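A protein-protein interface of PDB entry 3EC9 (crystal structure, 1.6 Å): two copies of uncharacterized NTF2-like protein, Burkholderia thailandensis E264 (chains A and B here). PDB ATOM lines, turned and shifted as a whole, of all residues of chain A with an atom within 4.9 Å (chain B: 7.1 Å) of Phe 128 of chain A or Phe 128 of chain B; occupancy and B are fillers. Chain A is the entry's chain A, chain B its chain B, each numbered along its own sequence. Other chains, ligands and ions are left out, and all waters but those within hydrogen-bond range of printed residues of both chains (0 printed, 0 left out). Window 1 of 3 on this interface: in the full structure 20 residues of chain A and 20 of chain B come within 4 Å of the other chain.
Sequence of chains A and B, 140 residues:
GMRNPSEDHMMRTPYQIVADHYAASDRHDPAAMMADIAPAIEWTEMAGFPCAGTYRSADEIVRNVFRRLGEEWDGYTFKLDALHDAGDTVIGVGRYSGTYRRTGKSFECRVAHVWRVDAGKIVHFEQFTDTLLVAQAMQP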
ATOM      1  N   MET A  46       0.622  19.821   6.682  1.00  0.00           N
ATOM      2  CA  MET A  46      -0.070  19.760   5.388  1.00  0.00           C
ATOM      3  C   MET A  46      -0.857  18.466   5.265  1.00  0.00           C
ATOM      4  O   MET A  46      -0.448  17.446   5.779  1.00  0.00           O
ATOM      5  CB  MET A  46       0.936  19.891   4.243  1.00  0.00           C
ATOM      6  CG  MET A  46       0.283  20.097   2.942  1.00  0.00           C
ATOM      7  SD  MET A  46       1.538  20.447   1.525  1.00  0.00           S
ATOM      8  CE  MET A  46       0.938  22.207   0.835  1.00  0.00           C
ATOM      9  N   VAL A  93      11.620  29.406   4.600  1.00  0.00           N
ATOM     10  CA  VAL A  93      11.776  28.507   3.474  1.00  0.00           C
ATOM     11  C   VAL A  93      13.030  27.673   3.684  1.00  0.00           C
ATOM     12  O   VAL A  93      14.056  28.168   4.171  1.00  0.00           O
ATOM     13  CB  VAL A  93      11.878  29.290   2.146  1.00  0.00           C
ATOM     14  CG1 VAL A  93      12.019  28.315   0.916  1.00  0.00           C
ATOM     15  CG2 VAL A  93      10.681  30.263   1.982  1.00  0.00           C
ATOM     16  N   ARG A 110      11.735  20.434  -0.651  1.00  0.00           N
ATOM     17  CA  ARG A 110      11.547  21.805  -0.250  1.00  0.00           C
ATOM     18  C   ARG A 110      10.336  21.952   0.664  1.00  0.00           C
ATOM     19  O   ARG A 110       9.395  21.121   0.675  1.00  0.00           O
ATOM     20  CB  ARG A 110      11.389  22.742  -1.462  1.00  0.00           C
ATOM     21  CG  ARG A 110      12.594  22.778  -2.337  1.00  0.00           C
ATOM     22  CD  ARG A 110      13.622  23.648  -1.782  1.00  0.00           C
ATOM     23  NE  ARG A 110      13.331  25.066  -1.979  1.00  0.00           N
ATOM     24  CZ  ARG A 110      13.990  26.044  -1.390  1.00  0.00           C
ATOM     25  NH1 ARG A 110      14.880  25.759  -0.461  1.00  0.00           N
ATOM     26  NH2 ARG A 110      13.767  27.306  -1.743  1.00  0.00           N
ATOM     27  N   VAL A 111      10.342  23.054   1.404  1.00  0.00           N
ATOM     28  CA  VAL A 111       9.268  23.405   2.301  1.00  0.00           C
ATOM     29  C   VAL A 111       9.241  24.896   2.562  1.00  0.00           C
ATOM     30  O   VAL A 111      10.287  25.556   2.636  1.00  0.00           O
ATOM     31  CB  VAL A 111       9.340  22.633   3.676  1.00  0.00           C
ATOM     32  CG1 VAL A 111      10.738  22.787   4.363  1.00  0.00           C
ATOM     33  CG2 VAL A 111       8.166  23.065   4.652  1.00  0.00           C
ATOM     34  N   ALA A 112       8.023  25.414   2.700  1.00  0.00           N
ATOM     35  CA  ALA A 112       7.778  26.753   3.197  1.00  0.00           C
ATOM     36  C   ALA A 112       6.864  26.647   4.439  1.00  0.00           C
ATOM     37  O   ALA A 112       5.964  25.790   4.487  1.00  0.00           O
ATOM     38  CB  ALA A 112       7.116  27.642   2.124  1.00  0.00           C
ATOM     39  N   VAL A 114       4.487  29.200   6.955  1.00  0.00           N
ATOM     40  CA  VAL A 114       3.896  30.527   7.153  1.00  0.00           C
ATOM     41  C   VAL A 114       3.502  30.621   8.622  1.00  0.00           C
ATOM     42  O   VAL A 114       2.797  29.742   9.143  1.00  0.00           O
ATOM     43  CB  VAL A 114       2.670  30.772   6.231  1.00  0.00           C
ATOM     44  CG1 VAL A 114       1.997  32.134   6.574  1.00  0.00           C
ATOM     45  CG2 VAL A 114       3.071  30.688   4.733  1.00  0.00           C
ATOM     46  N   GLU A 126       1.668  27.127   9.409  1.00  0.00           N
ATOM     47  CA  GLU A 126       1.199  26.235   8.340  1.00  0.00           C
ATOM     48  C   GLU A 126       2.349  25.791   7.490  1.00  0.00           C
ATOM     49  O   GLU A 126       3.134  26.598   7.042  1.00  0.00           O
ATOM     50  CB  GLU A 126       0.073  26.863   7.501  1.00  0.00           C
ATOM     51  CG  GLU A 126      -0.472  25.901   6.463  1.00  0.00           C
ATOM     52  CD  GLU A 126      -1.722  26.384   5.739  1.00  0.00           C
ATOM     53  OE1 GLU A 126      -2.127  27.569   5.896  1.00  0.00           O
ATOM     54  OE2 GLU A 126      -2.315  25.541   4.976  1.00  0.00           O
ATOM     55  N   GLN A 127       2.380  24.485   7.237  1.00  0.00           N
ATOM     56  CA  GLN A 127       3.393  23.822   6.471  1.00  0.00           C
ATOM     57  C   GLN A 127       2.970  23.637   5.008  1.00  0.00           C
ATOM     58  O   GLN A 127       1.843  23.229   4.743  1.00  0.00           O
ATOM     59  CB  GLN A 127       3.611  22.442   7.113  1.00  0.00           C
ATOM     60  CG  GLN A 127       4.602  21.531   6.414  1.00  0.00           C
ATOM     61  CD  GLN A 127       4.457  20.082   6.867  1.00  0.00           C
ATOM     62  OE1 GLN A 127       3.367  19.503   6.784  1.00  0.00           O
ATOM     63  NE2 GLN A 127       5.525  19.528   7.429  1.00  0.00           N
ATOM     64  N   PHE A 128       3.899  23.893   4.087  1.00  0.00           N
ATOM     65  CA  PHE A 128       3.701  23.621   2.669  1.00  0.00           C
ATOM     66  C   PHE A 128       4.928  22.884   2.140  1.00  0.00           C
ATOM     67  O   PHE A 128       6.004  23.493   2.015  1.00  0.00           O
ATOM     68  CB  PHE A 128       3.514  24.931   1.880  1.00  0.00           C
ATOM     69  CG  PHE A 128       2.401  25.828   2.418  1.00  0.00           C
ATOM     70  CD1 PHE A 128       2.609  26.682   3.493  1.00  0.00           C
ATOM     71  CD2 PHE A 128       1.150  25.823   1.787  1.00  0.00           C
ATOM     72  CE1 PHE A 128       1.550  27.477   3.941  1.00  0.00           C
ATOM     73  CE2 PHE A 128       0.152  26.628   2.210  1.00  0.00           C
ATOM     74  CZ  PHE A 128       0.359  27.459   3.284  1.00  0.00           C
ATOM     75  N   THR A 129       4.811  21.577   1.926  1.00  0.00           N
ATOM     76  CA  THR A 129       5.951  20.747   1.566  1.00  0.00           C
ATOM     77  C   THR A 129       5.601  19.722   0.505  1.00  0.00           C
ATOM     78  O   THR A 129       4.419  19.536   0.162  1.00  0.00           O
ATOM     79  CB  THR A 129       6.588  20.084   2.809  1.00  0.00           C
ATOM     80  OG1 THR A 129       7.909  19.569   2.482  1.00  0.00           O
ATOM     81  CG2 THR A 129       5.726  18.947   3.361  1.00  0.00           C
ATOM     82  N   ASP A 130       6.642  19.060  -0.017  1.00  0.00           N
ATOM     83  CA  ASP A 130       6.513  18.126  -1.164  1.00  0.00           C
ATOM     84  C   ASP A 130       6.068  16.778  -0.620  1.00  0.00           C
ATOM     85  O   ASP A 130       6.850  15.817  -0.413  1.00  0.00           O
ATOM     86  CB  ASP A 130       7.852  18.066  -1.898  1.00  0.00           C
ATOM     87  CG  ASP A 130       7.709  17.660  -3.359  1.00  0.00           C
ATOM     88  OD1 ASP A 130       6.821  16.843  -3.671  1.00  0.00           O
ATOM     89  OD2 ASP A 130       8.551  18.126  -4.185  1.00  0.00           O
ATOM     90  N   THR B  44      10.159  28.105 -10.642  1.00  0.00           N
ATOM     91  CA  THR B  44      10.254  26.744 -10.189  1.00  0.00           C
ATOM     92  C   THR B  44       8.890  26.126  -9.751  1.00  0.00           C
ATOM     93  O   THR B  44       8.247  26.551  -8.790  1.00  0.00           O
ATOM     94  CB  THR B  44      11.255  26.581  -9.035  1.00  0.00           C
ATOM     95  OG1 THR B  44      12.532  27.048  -9.492  1.00  0.00           O
ATOM     96  CG2 THR B  44      11.307  25.130  -8.561  1.00  0.00           C
ATOM     97  N   GLU B  45       8.471  25.111 -10.487  1.00  0.00           N
ATOM     98  CA  GLU B  45       7.336  24.266 -10.133  1.00  0.00           C
ATOM     99  C   GLU B  45       7.950  23.152  -9.243  1.00  0.00           C
ATOM    100  O   GLU B  45       9.064  22.675  -9.495  1.00  0.00           O
ATOM    101  CB  GLU B  45       6.695  23.661 -11.380  1.00  0.00           C
ATOM    102  CG  GLU B  45       6.006  24.689 -12.268  1.00  0.00           C
ATOM    103  CD  GLU B  45       4.719  25.162 -11.709  1.00  0.00           C
ATOM    104  OE1 GLU B  45       3.780  24.365 -11.590  1.00  0.00           O
ATOM    105  OE2 GLU B  45       4.601  26.359 -11.445  1.00  0.00           O
ATOM    106  N   MET B  46       7.246  22.821  -8.160  1.00  0.00           N
ATOM    107  CA  MET B  46       7.791  21.901  -7.175  1.00  0.00           C
ATOM    108  C   MET B  46       8.168  20.524  -7.744  1.00  0.00           C
ATOM    109  O   MET B  46       7.497  20.017  -8.611  1.00  0.00           O
ATOM    110  CB  MET B  46       6.794  21.736  -6.027  1.00  0.00           C
ATOM    111  CG  MET B  46       7.340  21.052  -4.863  1.00  0.00           C
ATOM    112  SD  MET B  46       6.137  21.003  -3.294  1.00  0.00           S
ATOM    113  CE  MET B  46       7.112  22.021  -1.925  1.00  0.00           C
ATOM    114  N   ILE B  91       4.570  36.636  -0.766  1.00  0.00           N
ATOM    115  CA  ILE B  91       4.166  35.227  -0.638  1.00  0.00           C
ATOM    116  C   ILE B  91       2.645  35.131  -0.792  1.00  0.00           C
ATOM    117  O   ILE B  91       1.885  35.670   0.022  1.00  0.00           O
ATOM    118  CB  ILE B  91       4.627  34.601   0.727  1.00  0.00           C
ATOM    119  CG1 ILE B  91       6.153  34.727   0.863  1.00  0.00           C
ATOM    120  CG2 ILE B  91       4.178  33.139   0.866  1.00  0.00           C
ATOM    121  CD1 ILE B  91       6.693  36.073   1.408  1.00  0.00           C
ATOM    122  N   GLY B  92       2.215  34.408  -1.826  1.00  0.00           N
ATOM    123  CA  GLY B  92       0.792  34.134  -2.054  1.00  0.00           C
ATOM    124  C   GLY B  92       0.425  32.802  -1.405  1.00  0.00           C
ATOM    125  O   GLY B  92       1.266  31.888  -1.357  1.00  0.00           O
ATOM    126  N   VAL B  93      -0.781  32.687  -0.844  1.00  0.00           N
ATOM    127  CA  VAL B  93      -1.221  31.430  -0.248  1.00  0.00           C
ATOM    128  C   VAL B  93      -2.639  31.218  -0.722  1.00  0.00           C
ATOM    129  O   VAL B  93      -3.430  32.164  -0.820  1.00  0.00           O
ATOM    130  CB  VAL B  93      -1.189  31.479   1.276  1.00  0.00           C
ATOM    131  CG1 VAL B  93      -1.738  30.152   1.859  1.00  0.00           C
ATOM    132  CG2 VAL B  93       0.217  31.828   1.813  1.00  0.00           C
ATOM    133  N   GLY B  94      -2.999  29.983  -1.037  1.00  0.00           N
ATOM    134  CA  GLY B  94      -4.369  29.698  -1.400  1.00  0.00           C
ATOM    135  C   GLY B  94      -4.579  28.225  -1.638  1.00  0.00           C
ATOM    136  O   GLY B  94      -3.913  27.395  -1.046  1.00  0.00           O
ATOM    137  N   TYR B  96      -5.457  25.135  -4.704  1.00  0.00           N
ATOM    138  CA  TYR B  96      -5.584  24.601  -6.031  1.00  0.00           C
ATOM    139  C   TYR B  96      -6.728  23.622  -6.059  1.00  0.00           C
ATOM    140  O   TYR B  96      -7.001  22.935  -5.069  1.00  0.00           O
ATOM    141  CB  TYR B  96      -4.367  23.790  -6.451  1.00  0.00           C
ATOM    142  CG  TYR B  96      -3.119  24.543  -6.803  1.00  0.00           C
ATOM    143  CD1 TYR B  96      -3.143  25.691  -7.620  1.00  0.00           C
ATOM    144  CD2 TYR B  96      -1.866  24.049  -6.435  1.00  0.00           C
ATOM    145  CE1 TYR B  96      -1.941  26.338  -7.985  1.00  0.00           C
ATOM    146  CE2 TYR B  96      -0.708  24.673  -6.776  1.00  0.00           C
ATOM    147  CZ  TYR B  96      -0.732  25.841  -7.541  1.00  0.00           C
ATOM    148  OH  TYR B  96       0.460  26.424  -7.897  1.00  0.00           O
ATOM    149  N   ARG B 110      -3.772  22.834  -0.610  1.00  0.00           N
ATOM    150  CA  ARG B 110      -3.151  24.109  -0.316  1.00  0.00           C
ATOM    151  C   ARG B 110      -1.903  24.341  -1.129  1.00  0.00           C
ATOM    152  O   ARG B 110      -1.237  23.401  -1.618  1.00  0.00           O
ATOM    153  CB  ARG B 110      -2.843  24.196   1.180  1.00  0.00           C
ATOM    154  CG  ARG B 110      -4.102  24.167   2.091  1.00  0.00           C
ATOM    155  CD  ARG B 110      -4.785  25.467   2.065  1.00  0.00           C
ATOM    156  NE  ARG B 110      -4.138  26.445   2.941  1.00  0.00           N
ATOM    157  CZ  ARG B 110      -4.402  27.747   2.934  1.00  0.00           C
ATOM    158  NH1 ARG B 110      -5.215  28.264   2.023  1.00  0.00           N
ATOM    159  NH2 ARG B 110      -3.860  28.544   3.839  1.00  0.00           N
ATOM    160  N   VAL B 111      -1.551  25.612  -1.260  1.00  0.00           N
ATOM    161  CA  VAL B 111      -0.353  26.010  -1.979  1.00  0.00           C
ATOM    162  C   VAL B 111       0.134  27.352  -1.436  1.00  0.00           C
ATOM    163  O   VAL B 111      -0.667  28.229  -1.095  1.00  0.00           O
ATOM    164  CB  VAL B 111      -0.547  26.082  -3.519  1.00  0.00           C
ATOM    165  CG1 VAL B 111      -1.719  26.970  -3.918  1.00  0.00           C
ATOM    166  CG2 VAL B 111       0.783  26.528  -4.192  1.00  0.00           C
ATOM    167  N   ALA B 112       1.457  27.491  -1.347  1.00  0.00           N
ATOM    168  CA  ALA B 112       2.108  28.776  -1.175  1.00  0.00           C
ATOM    169  C   ALA B 112       3.059  29.023  -2.358  1.00  0.00           C
ATOM    170  O   ALA B 112       3.702  28.065  -2.885  1.00  0.00           O
ATOM    171  CB  ALA B 112       2.884  28.854   0.153  1.00  0.00           C
ATOM    172  N   HIS B 113       3.122  30.286  -2.797  1.00  0.00           N
ATOM    173  CA  HIS B 113       4.020  30.751  -3.844  1.00  0.00           C
ATOM    174  C   HIS B 113       4.911  31.855  -3.303  1.00  0.00           C
ATOM    175  O   HIS B 113       4.420  32.831  -2.732  1.00  0.00           O
ATOM    176  CB  HIS B 113       3.270  31.369  -5.002  1.00  0.00           C
ATOM    177  CG  HIS B 113       2.242  30.484  -5.607  1.00  0.00           C
ATOM    178  ND1 HIS B 113       1.004  30.939  -5.988  1.00  0.00           N
ATOM    179  CD2 HIS B 113       2.295  29.180  -5.966  1.00  0.00           C
ATOM    180  CE1 HIS B 113       0.320  29.945  -6.522  1.00  0.00           C
ATOM    181  NE2 HIS B 113       1.090  28.878  -6.557  1.00  0.00           N
ATOM    182  N   VAL B 114       6.211  31.668  -3.461  1.00  0.00           N
ATOM    183  CA  VAL B 114       7.190  32.686  -3.063  1.00  0.00           C
ATOM    184  C   VAL B 114       7.740  33.396  -4.308  1.00  0.00           C
ATOM    185  O   VAL B 114       8.210  32.751  -5.254  1.00  0.00           O
ATOM    186  CB  VAL B 114       8.376  32.082  -2.243  1.00  0.00           C
ATOM    187  CG1 VAL B 114       9.419  33.180  -1.920  1.00  0.00           C
ATOM    188  CG2 VAL B 114       7.852  31.384  -0.975  1.00  0.00           C
ATOM    189  N   PHE B 125      10.020  32.804  -8.916  1.00  0.00           N
ATOM    190  CA  PHE B 125       8.767  32.197  -8.448  1.00  0.00           C
ATOM    191  C   PHE B 125       9.121  30.802  -7.976  1.00  0.00           C
ATOM    192  O   PHE B 125       9.868  30.071  -8.647  1.00  0.00           O
ATOM    193  CB  PHE B 125       7.755  32.074  -9.586  1.00  0.00           C
ATOM    194  CG  PHE B 125       6.595  31.161  -9.312  1.00  0.00           C
ATOM    195  CD1 PHE B 125       6.664  29.797  -9.619  1.00  0.00           C
ATOM    196  CD2 PHE B 125       5.439  31.663  -8.731  1.00  0.00           C
ATOM    197  CE1 PHE B 125       5.575  28.995  -9.373  1.00  0.00           C
ATOM    198  CE2 PHE B 125       4.325  30.833  -8.491  1.00  0.00           C
ATOM    199  CZ  PHE B 125       4.409  29.523  -8.815  1.00  0.00           C
ATOM    200  N   GLU B 126       8.567  30.416  -6.829  1.00  0.00           N
ATOM    201  CA  GLU B 126       8.693  29.030  -6.400  1.00  0.00           C
ATOM    202  C   GLU B 126       7.364  28.535  -5.803  1.00  0.00           C
ATOM    203  O   GLU B 126       6.762  29.215  -4.962  1.00  0.00           O
ATOM    204  CB  GLU B 126       9.906  28.799  -5.480  1.00  0.00           C
ATOM    205  CG  GLU B 126      10.069  27.303  -5.076  1.00  0.00           C
ATOM    206  CD  GLU B 126      11.289  27.012  -4.277  1.00  0.00           C
ATOM    207  OE1 GLU B 126      12.027  27.965  -3.879  1.00  0.00           O
ATOM    208  OE2 GLU B 126      11.589  25.790  -4.098  1.00  0.00           O
ATOM    209  N   GLN B 127       6.937  27.345  -6.218  1.00  0.00           N
ATOM    210  CA  GLN B 127       5.680  26.759  -5.810  1.00  0.00           C
ATOM    211  C   GLN B 127       5.927  25.721  -4.668  1.00  0.00           C
ATOM    212  O   GLN B 127       6.858  24.914  -4.740  1.00  0.00           O
ATOM    213  CB  GLN B 127       5.089  26.008  -7.013  1.00  0.00           C
ATOM    214  CG  GLN B 127       3.847  25.202  -6.758  1.00  0.00           C
ATOM    215  CD  GLN B 127       3.651  24.182  -7.901  1.00  0.00           C
ATOM    216  OE1 GLN B 127       4.535  23.329  -8.172  1.00  0.00           O
ATOM    217  NE2 GLN B 127       2.533  24.279  -8.578  1.00  0.00           N
ATOM    218  N   PHE B 128       5.060  25.751  -3.649  1.00  0.00           N
ATOM    219  CA  PHE B 128       5.077  24.784  -2.562  1.00  0.00           C
ATOM    220  C   PHE B 128       3.654  24.255  -2.368  1.00  0.00           C
ATOM    221  O   PHE B 128       2.811  24.958  -1.826  1.00  0.00           O
ATOM    222  CB  PHE B 128       5.558  25.405  -1.242  1.00  0.00           C
ATOM    223  CG  PHE B 128       6.909  26.101  -1.319  1.00  0.00           C
ATOM    224  CD1 PHE B 128       6.999  27.346  -1.875  1.00  0.00           C
ATOM    225  CD2 PHE B 128       8.059  25.478  -0.856  1.00  0.00           C
ATOM    226  CE1 PHE B 128       8.238  27.984  -1.963  1.00  0.00           C
ATOM    227  CE2 PHE B 128       9.296  26.098  -0.925  1.00  0.00           C
ATOM    228  CZ  PHE B 128       9.392  27.362  -1.496  1.00  0.00           C
ATOM    229  N   THR B 129       3.339  23.055  -2.855  1.00  0.00           N
ATOM    230  CA  THR B 129       1.989  22.527  -2.821  1.00  0.00           C
ATOM    231  C   THR B 129       1.929  21.064  -2.427  1.00  0.00           C
ATOM    232  O   THR B 129       2.970  20.391  -2.302  1.00  0.00           O
ATOM    233  CB  THR B 129       1.273  22.777  -4.161  1.00  0.00           C
ATOM    234  OG1 THR B 129      -0.157  22.602  -4.033  1.00  0.00           O
ATOM    235  CG2 THR B 129       1.837  21.887  -5.272  1.00  0.00           C
ATOM    236  N   ASP B 130       0.702  20.570  -2.234  1.00  0.00           N
ATOM    237  CA  ASP B 130       0.481  19.214  -1.724  1.00  0.00           C
ATOM    238  C   ASP B 130       0.550  18.249  -2.856  1.00  0.00           C
ATOM    239  O   ASP B 130      -0.439  17.780  -3.429  1.00  0.00           O
ATOM    240  CB  ASP B 130      -0.849  19.198  -0.969  1.00  0.00           C
ATOM    241  CG  ASP B 130      -0.931  18.079   0.073  1.00  0.00           C
ATOM    242  OD1 ASP B 130      -0.266  17.027  -0.087  1.00  0.00           O
ATOM    243  OD2 ASP B 130      -1.700  18.240   1.061  1.00  0.00           O
ATOM    244  N   THR B 131       1.780  17.958  -3.228  1.00  0.00           N
ATOM    245  CA  THR B 131       2.012  17.122  -4.392  1.00  0.00           C
ATOM    246  C   THR B 131       1.417  15.712  -4.296  1.00  0.00           C
ATOM    247  O   THR B 131       1.060  15.102  -5.315  1.00  0.00           O
ATOM    248  CB  THR B 131       3.527  17.097  -4.689  1.00  0.00           C
ATOM    249  OG1 THR B 131       4.198  16.733  -3.503  1.00  0.00           O
ATOM    250  CG2 THR B 131       4.022  18.486  -5.154  1.00  0.00           C
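Of the printed residues of chain B, Phe 128 of chain A touches Val 93, Arg 110, Val 111, Ala 112 and Phe 128. Printed residues of chain B within 4 Å of Thr 129 of chain A: Met 46 (3.7 Å) and Thr 129 (3.0 Å). Of the printed residues of chain A, Met 46 of chain B touches Arg 110, Thr 129 and Asp 130. Of the printed residues of chain A, Arg 110 of chain B touches Met 46, Glu 126 and Phe 128. Printed residues of chain A within 4 Å of Phe 128 of chain B: Val 93 (3.7 Å), Arg 110 (3.99 Å), Val 111 (3.7 Å), Ala 112 (3.6 Å) and Phe 128 (3.8 Å). Of the printed residues of chain A, Thr 129 of chain B touches Met 46 (3.6 Å) and Thr 129 (3.0 Å). The nearest printed residue of chain B that does not touch Asp 130 of chain A is Thr 129 of chain B (4.4 Å).
N of Gly 94 of chain B lies within hydrogen-bond range of O of Val 111 of chain B (2.9 Å). OE1 of Gln 127 of chain A lies within hydrogen-bond range of N of Met 46 of chain A. The backbone NH (N) of Thr 129 of chain A sits at hydrogen-bond distance from the side-chain sulfur (SD) of Met 46 of chain A, at 3.5 Å. The backbone NH of Met 46 of chain B is in hydrogen-bond range of the side-chain amide oxygen of Gln 127 of chain B (2.8 Å). The backbone carbonyl oxygen (O) of Arg 110 of chain B sits at hydrogen-bond distance from the backbone NH (N) of Asp 130 of chain B (3.5 Å). The backbone carbonyl oxygen (O) of Val 114 of chain B is in hydrogen-bond range of the backbone NH (N) of Glu 126 of chain B (2.8 Å).
Arg 110 of chain A touches Glu 126 of chain B, and with the chains exchanged Glu 126 of chain A touches Arg 110 of chain B. Arg 110 of chain A touches Phe 128 of chain B, and with the chains exchanged Phe 128 of chain A touches Arg 110 of chain B. Val 111 of chain A touches Phe 128 of chain B, and with the chains exchanged Phe 128 of chain A touches Val 111 of chain B. Phe 128 of chain B touches its own counterpart, Phe 128 of chain A. Positions printed for both chains: 46, 93, 110, 111, 112, 114, 126, 127, 128, 129 and 130. Of the 19 pairs that touch across the chains among the printed residues, 18 have their exchanged pair printed and touching as well.
Hydrophobic or aromatic side chains of chain A within 4 Å of the printed part of chain B: Met 46, Val 93, Ala 112 and Phe 128. Of the 20 printed residues of chain B, 10 touch a printed residue of chain A. Hydrophobic or aromatic side chains of chain B that line the printed part of chain A: Met 46, Val 93, Ala 112 and Phe 128. Along chain B the printed residues that touch a printed residue of chain A span positions 46 to 131.
Met 46 of chain A touches Asp 130 of chain B. Phe 128 of chain B touches Val 93 of chain A. CE of Met 46 of chain B touches O of Arg 110 of chain A, at 3.6 Å. Phe 128 of chain B touches Val 111 of chain A (CD2 to C, 3.7 Å). CZ of Phe 128 of chain A touches CG1 of Val 93 of chain B, at 3.7 Å. Phe 128 of chain A touches Arg 110 of chain B. Phe 128 of chain A touches Val 111 of chain B (CD2 to C, 3.7 Å). CD2 of Phe 128 of chain A touches N of Ala 112 of chain B, 3.6 Å away. Phe 128 of chain A touches Phe 128 of chain B. Met 46 of chain B touches Thr 129 of chain A.
OE1 of Glu 126 of chain A is in salt-bridge range of NH2 of Arg 110 of chain B, 2.9 Å away. The backbone carbonyl oxygen (O) of Thr 129 of chain B lies close to the backbone carbonyl oxygen (O) of Thr 129 of chain A, 3.0 Å away. The side-chain hydroxyl (OG1) of Thr 131 of chain B is in hydrogen-bond range of the side-chain carboxylate (OD1) of Asp 130 of chain A, 2.6 Å away. OE1 of Glu 126 of chain B is in salt-bridge range of NH2 of Arg 110 of chain A, at 2.8 Å.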
